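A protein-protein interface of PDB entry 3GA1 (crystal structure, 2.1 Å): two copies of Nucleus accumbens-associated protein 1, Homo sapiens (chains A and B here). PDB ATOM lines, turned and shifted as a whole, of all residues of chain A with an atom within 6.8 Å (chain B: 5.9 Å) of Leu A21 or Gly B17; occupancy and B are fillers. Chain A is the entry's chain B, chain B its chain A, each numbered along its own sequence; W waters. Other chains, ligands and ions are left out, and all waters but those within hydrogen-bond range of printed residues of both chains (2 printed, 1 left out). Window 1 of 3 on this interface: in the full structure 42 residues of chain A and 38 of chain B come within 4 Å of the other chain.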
ATOM      1  N   ASN A  15       8.252   7.186  -0.957  1.00  0.00           N
ATOM      2  CA  ASN A  15       7.228   6.590  -1.780  1.00  0.00           C
ATOM      3  C   ASN A  15       7.032   5.112  -1.447  1.00  0.00           C
ATOM      4  O   ASN A  15       6.735   4.274  -2.310  1.00  0.00           O
ATOM      5  CB  ASN A  15       7.602   6.801  -3.240  1.00  0.00           C
ATOM      6  CG  ASN A  15       7.634   8.273  -3.612  1.00  0.00           C
ATOM      7  OD1 ASN A  15       6.696   9.010  -3.327  1.00  0.00           O
ATOM      8  ND2 ASN A  15       8.716   8.705  -4.236  1.00  0.00           N
ATOM      9  N   PHE A  16       7.164   4.809  -0.167  1.00  0.00           N
ATOM     10  CA  PHE A  16       6.950   3.451   0.340  1.00  0.00           C
ATOM     11  C   PHE A  16       5.515   2.945   0.073  1.00  0.00           C
ATOM     12  O   PHE A  16       5.301   1.819  -0.418  1.00  0.00           O
ATOM     13  CB  PHE A  16       7.237   3.461   1.839  1.00  0.00           C
ATOM     14  CG  PHE A  16       7.281   2.095   2.468  1.00  0.00           C
ATOM     15  CD1 PHE A  16       8.309   1.207   2.176  1.00  0.00           C
ATOM     16  CD2 PHE A  16       6.305   1.715   3.370  1.00  0.00           C
ATOM     17  CE1 PHE A  16       8.352  -0.042   2.771  1.00  0.00           C
ATOM     18  CE2 PHE A  16       6.344   0.465   3.984  1.00  0.00           C
ATOM     19  CZ  PHE A  16       7.370  -0.412   3.687  1.00  0.00           C
ATOM     20  N   GLY A  17       4.530   3.772   0.409  1.00  0.00           N
ATOM     21  CA  GLY A  17       3.115   3.388   0.232  1.00  0.00           C
ATOM     22  C   GLY A  17       2.772   3.026  -1.201  1.00  0.00           C
ATOM     23  O   GLY A  17       2.010   2.075  -1.439  1.00  0.00           O
ATOM     24  N   ASN A  18       3.303   3.788  -2.155  1.00  0.00           N
ATOM     25  CA  ASN A  18       3.111   3.507  -3.580  1.00  0.00           C
ATOM     26  C   ASN A  18       3.546   2.066  -3.937  1.00  0.00           C
ATOM     27  O   ASN A  18       2.883   1.364  -4.712  1.00  0.00           O
ATOM     28  CB  ASN A  18       3.871   4.521  -4.476  1.00  0.00           C
ATOM     29  CG  ASN A  18       3.266   5.941  -4.446  1.00  0.00           C
ATOM     30  OD1 ASN A  18       2.138   6.146  -3.985  1.00  0.00           O
ATOM     31  ND2 ASN A  18       4.037   6.932  -4.929  1.00  0.00           N
ATOM     32  N   SER A  19       4.670   1.621  -3.387  1.00  0.00           N
ATOM     33  CA  SER A  19       5.150   0.299  -3.735  1.00  0.00           C
ATOM     34  C   SER A  19       4.363  -0.757  -2.966  1.00  0.00           C
ATOM     35  O   SER A  19       4.072  -1.799  -3.492  1.00  0.00           O
ATOM     36  CB  SER A  19       6.655   0.172  -3.479  1.00  0.00           C
ATOM     37  OG  SER A  19       6.904   0.338  -2.110  1.00  0.00           O
ATOM     38  N   ILE A  20       3.982  -0.471  -1.734  1.00  0.00           N
ATOM     39  CA  ILE A  20       3.291  -1.466  -0.914  1.00  0.00           C
ATOM     40  C   ILE A  20       1.876  -1.722  -1.450  1.00  0.00           C
ATOM     41  O   ILE A  20       1.440  -2.873  -1.586  1.00  0.00           O
ATOM     42  CB  ILE A  20       3.243  -1.046   0.560  1.00  0.00           C
ATOM     43  CG1 ILE A  20       4.657  -1.015   1.161  1.00  0.00           C
ATOM     44  CG2 ILE A  20       2.408  -1.997   1.369  1.00  0.00           C
ATOM     45  CD1 ILE A  20       5.400  -2.354   1.072  1.00  0.00           C
ATOM     46  N   LEU A  21       1.167  -0.658  -1.795  1.00  0.00           N
ATOM     47  CA  LEU A  21      -0.146  -0.825  -2.378  1.00  0.00           C
ATOM     48  C   LEU A  21      -0.067  -1.653  -3.656  1.00  0.00           C
ATOM     49  O   LEU A  21      -0.940  -2.453  -3.947  1.00  0.00           O
ATOM     50  CB  LEU A  21      -0.768   0.526  -2.679  1.00  0.00           C
ATOM     51  CG  LEU A  21      -2.182   0.392  -3.211  1.00  0.00           C
ATOM     52  CD1 LEU A  21      -3.090  -0.155  -2.117  1.00  0.00           C
ATOM     53  CD2 LEU A  21      -2.670   1.758  -3.738  1.00  0.00           C
ATOM     54  N   GLU A  22       0.988  -1.450  -4.430  1.00  0.00           N
ATOM     55  CA  GLU A  22       1.203  -2.238  -5.632  1.00  0.00           C
ATOM     56  C   GLU A  22       1.332  -3.736  -5.299  1.00  0.00           C
ATOM     57  O   GLU A  22       0.796  -4.554  -6.008  1.00  0.00           O
ATOM     58  CB  GLU A  22       2.434  -1.712  -6.353  1.00  0.00           C
ATOM     59  CG  GLU A  22       2.542  -2.069  -7.776  1.00  0.00           C
ATOM     60  CD  GLU A  22       3.711  -1.329  -8.417  1.00  0.00           C
ATOM     61  OE1 GLU A  22       3.776  -0.076  -8.297  1.00  0.00           O
ATOM     62  OE2 GLU A  22       4.576  -1.994  -9.007  1.00  0.00           O
ATOM     63  N   CYS A  23       2.002  -4.119  -4.212  1.00  0.00           N
ATOM     64  CA  CYS A  23       2.175  -5.441  -3.646  1.00  0.00           C
ATOM     65  C   CYS A  23       0.803  -5.963  -3.215  1.00  0.00           C
ATOM     66  O   CYS A  23       0.455  -7.109  -3.503  1.00  0.00           O
ATOM     67  CB  CYS A  23       3.130  -5.445  -2.475  1.00  0.00           C
ATOM     68  SG  CYS A  23       3.461  -7.109  -1.929  1.00  0.00           S
ATOM     69  N   LEU A  24       0.020  -5.102  -2.556  1.00  0.00           N
ATOM     70  CA  LEU A  24      -1.324  -5.467  -2.137  1.00  0.00           C
ATOM     71  C   LEU A  24      -2.192  -5.801  -3.343  1.00  0.00           C
ATOM     72  O   LEU A  24      -2.991  -6.711  -3.309  1.00  0.00           O
ATOM     73  CB  LEU A  24      -1.977  -4.341  -1.330  1.00  0.00           C
ATOM     74  CG  LEU A  24      -1.297  -3.945  -0.014  1.00  0.00           C
ATOM     75  CD1 LEU A  24      -2.149  -2.994   0.825  1.00  0.00           C
ATOM     76  CD2 LEU A  24      -0.936  -5.147   0.792  1.00  0.00           C
ATOM     77  N   ASN A  25      -2.038  -5.058  -4.415  1.00  0.00           N
ATOM     78  CA  ASN A  25      -2.815  -5.348  -5.604  1.00  0.00           C
ATOM     79  C   ASN A  25      -2.478  -6.716  -6.184  1.00  0.00           C
ATOM     80  O   ASN A  25      -3.370  -7.470  -6.563  1.00  0.00           O
ATOM     81  CB  ASN A  25      -2.590  -4.290  -6.657  1.00  0.00           C
ATOM     82  CG  ASN A  25      -3.664  -4.300  -7.711  1.00  0.00           C
ATOM     83  OD1 ASN A  25      -4.832  -4.635  -7.441  1.00  0.00           O
ATOM     84  ND2 ASN A  25      -3.287  -3.952  -8.913  1.00  0.00           N
ATOM     85  N   GLU A  26      -1.181  -7.023  -6.248  1.00  0.00           N
ATOM     86  CA  GLU A  26      -0.704  -8.310  -6.754  1.00  0.00           C
ATOM     87  C   GLU A  26      -1.206  -9.437  -5.865  1.00  0.00           C
ATOM     88  O   GLU A  26      -1.624 -10.459  -6.361  1.00  0.00           O
ATOM     89  CB  GLU A  26       0.835  -8.325  -6.823  1.00  0.00           C
ATOM     90  CG  GLU A  26       1.391  -7.291  -7.824  1.00  0.00           C
ATOM     91  CD  GLU A  26       2.902  -6.996  -7.663  1.00  0.00           C
ATOM     92  OE1 GLU A  26       3.544  -7.497  -6.687  1.00  0.00           O
ATOM     93  OE2 GLU A  26       3.442  -6.234  -8.519  1.00  0.00           O
ATOM     94  N   VAL A  51      -8.315  -2.100   2.509  1.00  0.00           N
ATOM     95  CA  VAL A  51      -8.105  -1.315   1.301  1.00  0.00           C
ATOM     96  C   VAL A  51      -9.453  -0.765   0.800  1.00  0.00           C
ATOM     97  O   VAL A  51      -9.530   0.362   0.357  1.00  0.00           O
ATOM     98  CB  VAL A  51      -7.410  -2.135   0.173  1.00  0.00           C
ATOM     99  CG1 VAL A  51      -7.370  -1.352  -1.105  1.00  0.00           C
ATOM    100  CG2 VAL A  51      -5.958  -2.520   0.592  1.00  0.00           C
ATOM    101  N   PHE A  88      -9.404   0.449  -8.989  1.00  0.00           N
ATOM    102  CA  PHE A  88      -9.084   1.817  -8.621  1.00  0.00           C
ATOM    103  C   PHE A  88      -8.661   1.892  -7.155  1.00  0.00           C
ATOM    104  O   PHE A  88      -7.714   2.610  -6.805  1.00  0.00           O
ATOM    105  CB  PHE A  88     -10.250   2.785  -8.898  1.00  0.00           C
ATOM    106  CG  PHE A  88     -10.102   4.100  -8.190  1.00  0.00           C
ATOM    107  CD1 PHE A  88      -9.398   5.142  -8.767  1.00  0.00           C
ATOM    108  CD2 PHE A  88     -10.635   4.277  -6.930  1.00  0.00           C
ATOM    109  CE1 PHE A  88      -9.245   6.342  -8.108  1.00  0.00           C
ATOM    110  CE2 PHE A  88     -10.492   5.464  -6.271  1.00  0.00           C
ATOM    111  CZ  PHE A  88      -9.789   6.508  -6.853  1.00  0.00           C
ATOM    112  N   CYS A  89      -9.345   1.155  -6.291  1.00  0.00           N
ATOM    113  CA  CYS A  89      -9.049   1.233  -4.853  1.00  0.00           C
ATOM    114  C   CYS A  89      -7.615   0.776  -4.537  1.00  0.00           C
ATOM    115  O   CYS A  89      -7.089   1.069  -3.455  1.00  0.00           O
ATOM    116  CB  CYS A  89     -10.016   0.374  -4.054  1.00  0.00           C
ATOM    117  SG  CYS A  89     -11.708   1.019  -3.994  1.00  0.00           S
ATOM    118  N   TYR A  90      -7.032   0.020  -5.465  1.00  0.00           N
ATOM    119  CA  TYR A  90      -5.724  -0.590  -5.275  1.00  0.00           C
ATOM    120  C   TYR A  90      -4.649   0.067  -6.129  1.00  0.00           C
ATOM    121  O   TYR A  90      -3.512  -0.372  -6.086  1.00  0.00           O
ATOM    122  CB  TYR A  90      -5.766  -2.069  -5.655  1.00  0.00           C
ATOM    123  CG  TYR A  90      -6.290  -2.999  -4.574  1.00  0.00           C
ATOM    124  CD1 TYR A  90      -7.651  -3.227  -4.419  1.00  0.00           C
ATOM    125  CD2 TYR A  90      -5.413  -3.662  -3.721  1.00  0.00           C
ATOM    126  CE1 TYR A  90      -8.119  -4.072  -3.432  1.00  0.00           C
ATOM    127  CE2 TYR A  90      -5.872  -4.515  -2.754  1.00  0.00           C
ATOM    128  CZ  TYR A  90      -7.214  -4.719  -2.611  1.00  0.00           C
ATOM    129  OH  TYR A  90      -7.645  -5.582  -1.655  1.00  0.00           O
ATOM    130  N   THR A  91      -5.011   1.072  -6.918  1.00  0.00           N
ATOM    131  CA  THR A  91      -4.091   1.668  -7.875  1.00  0.00           C
ATOM    132  C   THR A  91      -4.221   3.179  -7.953  1.00  0.00           C
ATOM    133  O   THR A  91      -3.261   3.863  -8.295  1.00  0.00           O
ATOM    134  CB  THR A  91      -4.304   1.115  -9.308  1.00  0.00           C
ATOM    135  OG1 THR A  91      -5.601   1.501  -9.813  1.00  0.00           O
ATOM    136  CG2 THR A  91      -4.166  -0.404  -9.344  1.00  0.00           C
ATOM    137  N   GLY A  92      -5.414   3.708  -7.694  1.00  0.00           N
ATOM    138  CA  GLY A  92      -5.628   5.146  -7.836  1.00  0.00           C
ATOM    139  C   GLY A  92      -5.782   5.510  -9.295  1.00  0.00           C
ATOM    140  O   GLY A  92      -5.743   6.678  -9.685  1.00  0.00           O
ATOM    141  N   ILE B  13      -4.645   9.275  -9.797  1.00  0.00           N
ATOM    142  CA  ILE B  13      -4.340  10.062  -8.616  1.00  0.00           C
ATOM    143  C   ILE B  13      -2.885   9.823  -8.228  1.00  0.00           C
ATOM    144  O   ILE B  13      -2.495   8.696  -7.928  1.00  0.00           O
ATOM    145  CB  ILE B  13      -5.270   9.708  -7.456  1.00  0.00           C
ATOM    146  CG1 ILE B  13      -6.718   9.999  -7.851  1.00  0.00           C
ATOM    147  CG2 ILE B  13      -4.891  10.484  -6.205  1.00  0.00           C
ATOM    148  CD1 ILE B  13      -7.713   9.549  -6.828  1.00  0.00           C
ATOM    149  N   PRO B  14      -2.069  10.881  -8.304  1.00  0.00           N
ATOM    150  CA  PRO B  14      -0.662  10.828  -7.925  1.00  0.00           C
ATOM    151  C   PRO B  14      -0.441  10.342  -6.487  1.00  0.00           C
ATOM    152  O   PRO B  14      -1.179  10.714  -5.572  1.00  0.00           O
ATOM    153  CB  PRO B  14      -0.189  12.276  -8.089  1.00  0.00           C
ATOM    154  CG  PRO B  14      -1.099  12.884  -9.065  1.00  0.00           C
ATOM    155  CD  PRO B  14      -2.440  12.184  -8.890  1.00  0.00           C
ATOM    156  N   ASN B  15       0.571   9.502  -6.302  1.00  0.00           N
ATOM    157  CA  ASN B  15       0.971   9.059  -4.967  1.00  0.00           C
ATOM    158  C   ASN B  15      -0.197   8.536  -4.170  1.00  0.00           C
ATOM    159  O   ASN B  15      -0.336   8.791  -2.976  1.00  0.00           O
ATOM    160  CB  ASN B  15       1.659  10.193  -4.239  1.00  0.00           C
ATOM    161  CG  ASN B  15       2.926  10.596  -4.933  1.00  0.00           C
ATOM    162  OD1 ASN B  15       3.781   9.759  -5.174  1.00  0.00           O
ATOM    163  ND2 ASN B  15       3.029  11.860  -5.327  1.00  0.00           N
ATOM    164  N   PHE B  16      -1.025   7.769  -4.855  1.00  0.00           N
ATOM    165  CA  PHE B  16      -2.194   7.180  -4.252  1.00  0.00           C
ATOM    166  C   PHE B  16      -1.822   6.155  -3.200  1.00  0.00           C
ATOM    167  O   PHE B  16      -2.437   6.088  -2.131  1.00  0.00           O
ATOM    168  CB  PHE B  16      -3.032   6.505  -5.333  1.00  0.00           C
ATOM    169  CG  PHE B  16      -4.349   6.023  -4.845  1.00  0.00           C
ATOM    170  CD1 PHE B  16      -5.377   6.916  -4.595  1.00  0.00           C
ATOM    171  CD2 PHE B  16      -4.575   4.674  -4.656  1.00  0.00           C
ATOM    172  CE1 PHE B  16      -6.597   6.469  -4.165  1.00  0.00           C
ATOM    173  CE2 PHE B  16      -5.774   4.223  -4.226  1.00  0.00           C
ATOM    174  CZ  PHE B  16      -6.799   5.118  -3.975  1.00  0.00           C
ATOM    175  N   GLY B  17      -0.842   5.319  -3.514  1.00  0.00           N
ATOM    176  CA  GLY B  17      -0.395   4.317  -2.538  1.00  0.00           C
ATOM    177  C   GLY B  17       0.113   4.959  -1.254  1.00  0.00           C
ATOM    178  O   GLY B  17      -0.182   4.501  -0.156  1.00  0.00           O
ATOM    179  N   ASN B  18       0.872   6.033  -1.384  1.00  0.00           N
ATOM    180  CA  ASN B  18       1.357   6.737  -0.216  1.00  0.00           C
ATOM    181  C   ASN B  18       0.217   7.084   0.758  1.00  0.00           C
ATOM    182  O   ASN B  18       0.361   6.880   1.959  1.00  0.00           O
ATOM    183  CB  ASN B  18       2.143   7.994  -0.618  1.00  0.00           C
ATOM    184  CG  ASN B  18       3.507   7.673  -1.218  1.00  0.00           C
ATOM    185  OD1 ASN B  18       4.009   6.549  -1.131  1.00  0.00           O
ATOM    186  ND2 ASN B  18       4.100   8.662  -1.852  1.00  0.00           N
ATOM    187  N   SER B  19      -0.934   7.585   0.295  1.00  0.00           N
ATOM    188  CA  SER B  19      -2.144   7.994   1.024  1.00  0.00           C
ATOM    189  C   SER B  19      -2.850   6.770   1.617  1.00  0.00           C
ATOM    190  O   SER B  19      -3.242   6.764   2.801  1.00  0.00           O
ATOM    191  CB  SER B  19      -3.097   8.813   0.145  1.00  0.00           C
ATOM    192  OG  SER B  19      -3.910   7.968  -0.636  1.00  0.00           O
ATOM    193  N   ILE B  20      -2.998   5.731   0.820  1.00  0.00           N
ATOM    194  CA  ILE B  20      -3.692   4.551   1.282  1.00  0.00           C
ATOM    195  C   ILE B  20      -2.943   3.861   2.435  1.00  0.00           C
ATOM    196  O   ILE B  20      -3.563   3.453   3.426  1.00  0.00           O
ATOM    197  CB  ILE B  20      -3.942   3.564   0.139  1.00  0.00           C
ATOM    198  CG1 ILE B  20      -4.848   4.207  -0.914  1.00  0.00           C
ATOM    199  CG2 ILE B  20      -4.631   2.317   0.674  1.00  0.00           C
ATOM    200  CD1 ILE B  20      -6.062   4.946  -0.315  1.00  0.00           C
ATOM    201  N   LEU B  21      -1.625   3.732   2.318  1.00  0.00           N
ATOM    202  CA  LEU B  21      -0.863   3.104   3.410  1.00  0.00           C
ATOM    203  C   LEU B  21      -0.968   3.934   4.685  1.00  0.00           C
ATOM    204  O   LEU B  21      -1.086   3.386   5.747  1.00  0.00           O
ATOM    205  CB  LEU B  21       0.599   2.891   3.044  1.00  0.00           C
ATOM    206  CG  LEU B  21       1.322   2.015   4.066  1.00  0.00           C
ATOM    207  CD1 LEU B  21       0.795   0.580   4.048  1.00  0.00           C
ATOM    208  CD2 LEU B  21       2.849   2.061   3.814  1.00  0.00           C
ATOM    209  N   GLU B  22      -0.964   5.254   4.585  1.00  0.00           N
ATOM    210  CA  GLU B  22      -1.236   6.086   5.775  1.00  0.00           C
ATOM    211  C   GLU B  22      -2.604   5.747   6.421  1.00  0.00           C
ATOM    212  O   GLU B  22      -2.718   5.606   7.647  1.00  0.00           O
ATOM    213  CB  GLU B  22      -1.158   7.569   5.395  1.00  0.00           C
ATOM    214  CG  GLU B  22      -0.798   8.469   6.534  1.00  0.00           C
ATOM    215  CD  GLU B  22      -0.900   9.943   6.180  1.00  0.00           C
ATOM    216  OE1 GLU B  22      -1.181  10.287   5.003  1.00  0.00           O
ATOM    217  OE2 GLU B  22      -0.704  10.765   7.091  1.00  0.00           O
HETATM  218  O   HOH W   1       4.985   6.607   1.892  1.00  0.00           O
HETATM  219  O   HOH W   2       5.782  11.772  -3.254  1.00  0.00           O
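Asn B15 touches its own counterpart, Asn A15.
Asn A15 touches Asn B18, and with the chains exchanged Asn A18 touches Asn B15.
Gly A17 touches Asn B18, and with the chains exchanged Asn A18 touches Gly B17.
Asn B18 touches its own counterpart, Asn A18.
Of chain B, only Phe B16 (3.6 Å) and Gly B17 (3.6 Å) come within 4 Å of Leu A21.
Gly B17 touches three residues of chain A.
Printed residues of chain B within 4 Å of Thr A91: Phe B16.
Of the printed residues of chain A, Asn B18 touches Asn A15, Phe A16, Gly A17 and Asn A18.
Of the printed residues of chain A, Leu B21 touches Phe A16 and Gly A17.
Of the printed residues of chain B, Asn A15 touches Asn B15 and Asn B18.
Of the printed residues of chain A, Ile B13 touches Phe A88 (3.7 Å) and Gly A92 (2.8 Å).
The nearest residue of chain A that does not touch Gly B17 is Thr A91 (5.6 Å).
Water W2 bridges OD1 of Asn A15 and OD1 of Asn B15.
Water W1 lies within hydrogen-bond range of OD1 of Asn B18, N of Gly A17 and N of Phe A16.
O of Phe B16 lies within hydrogen-bond range of OG of Ser B19, at 2.8 Å.
The backbone carbonyl oxygen of Phe A16 is in hydrogen-bond range of the side-chain hydroxyl of Ser A19 (2.8 Å).
Asn A15 touches Asn B15.
N of Phe A16 touches OD1 of Asn B18 (3.7 Å).
CB of Leu B21 touches CA of Gly A17 (3.8 Å).
Phe B16 touches Asn A18 (N to OD1, 3.7 Å).
CD2 of Leu A21 touches CD2 of Phe B16 (3.6 Å).
CZ of Phe A88 touches CD1 of Ile B13 (3.7 Å).
O of Phe A88 touches CE2 of Phe B16 (3.6 Å).
O of Cys A89 touches CE2 of Phe B16, 3.5 Å away.
Thr A91 touches Phe B16.
Phe B16 touches Gly A92.
OD1 of Asn A18 lies within hydrogen-bond range of N of Asn B18, at 2.9 Å.
N of Ile B13 lies within hydrogen-bond range of O of Gly A92.
The backbone NH of Gly A17 sits at hydrogen-bond distance from the side-chain amide oxygen of Asn B18 (3.2 Å).
The side-chain amide oxygen of Asn A18 sits at hydrogen-bond distance from the backbone NH of Gly B17 (3.1 Å).
ND2 of Asn B18 is in hydrogen-bond range of OD1 of Asn A15 (3.0 Å).
OD1 of Asn B15 lies within hydrogen-bond range of ND2 of Asn A18.
Of the 18 printed residues of chain A, 9 touch a printed residue of chain B.
Hydrophobic or aromatic side chains of chain A within 4 Å of the printed part of chain B: Phe A16, Leu A21 and Phe A88.
Of the 10 printed residues of chain B, 6 touch a printed residue of chain A.
Hydrophobic or aromatic side chains of chain B within 4 Å of the printed part of chain A: Ile B13, Phe B16 and Leu B21.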
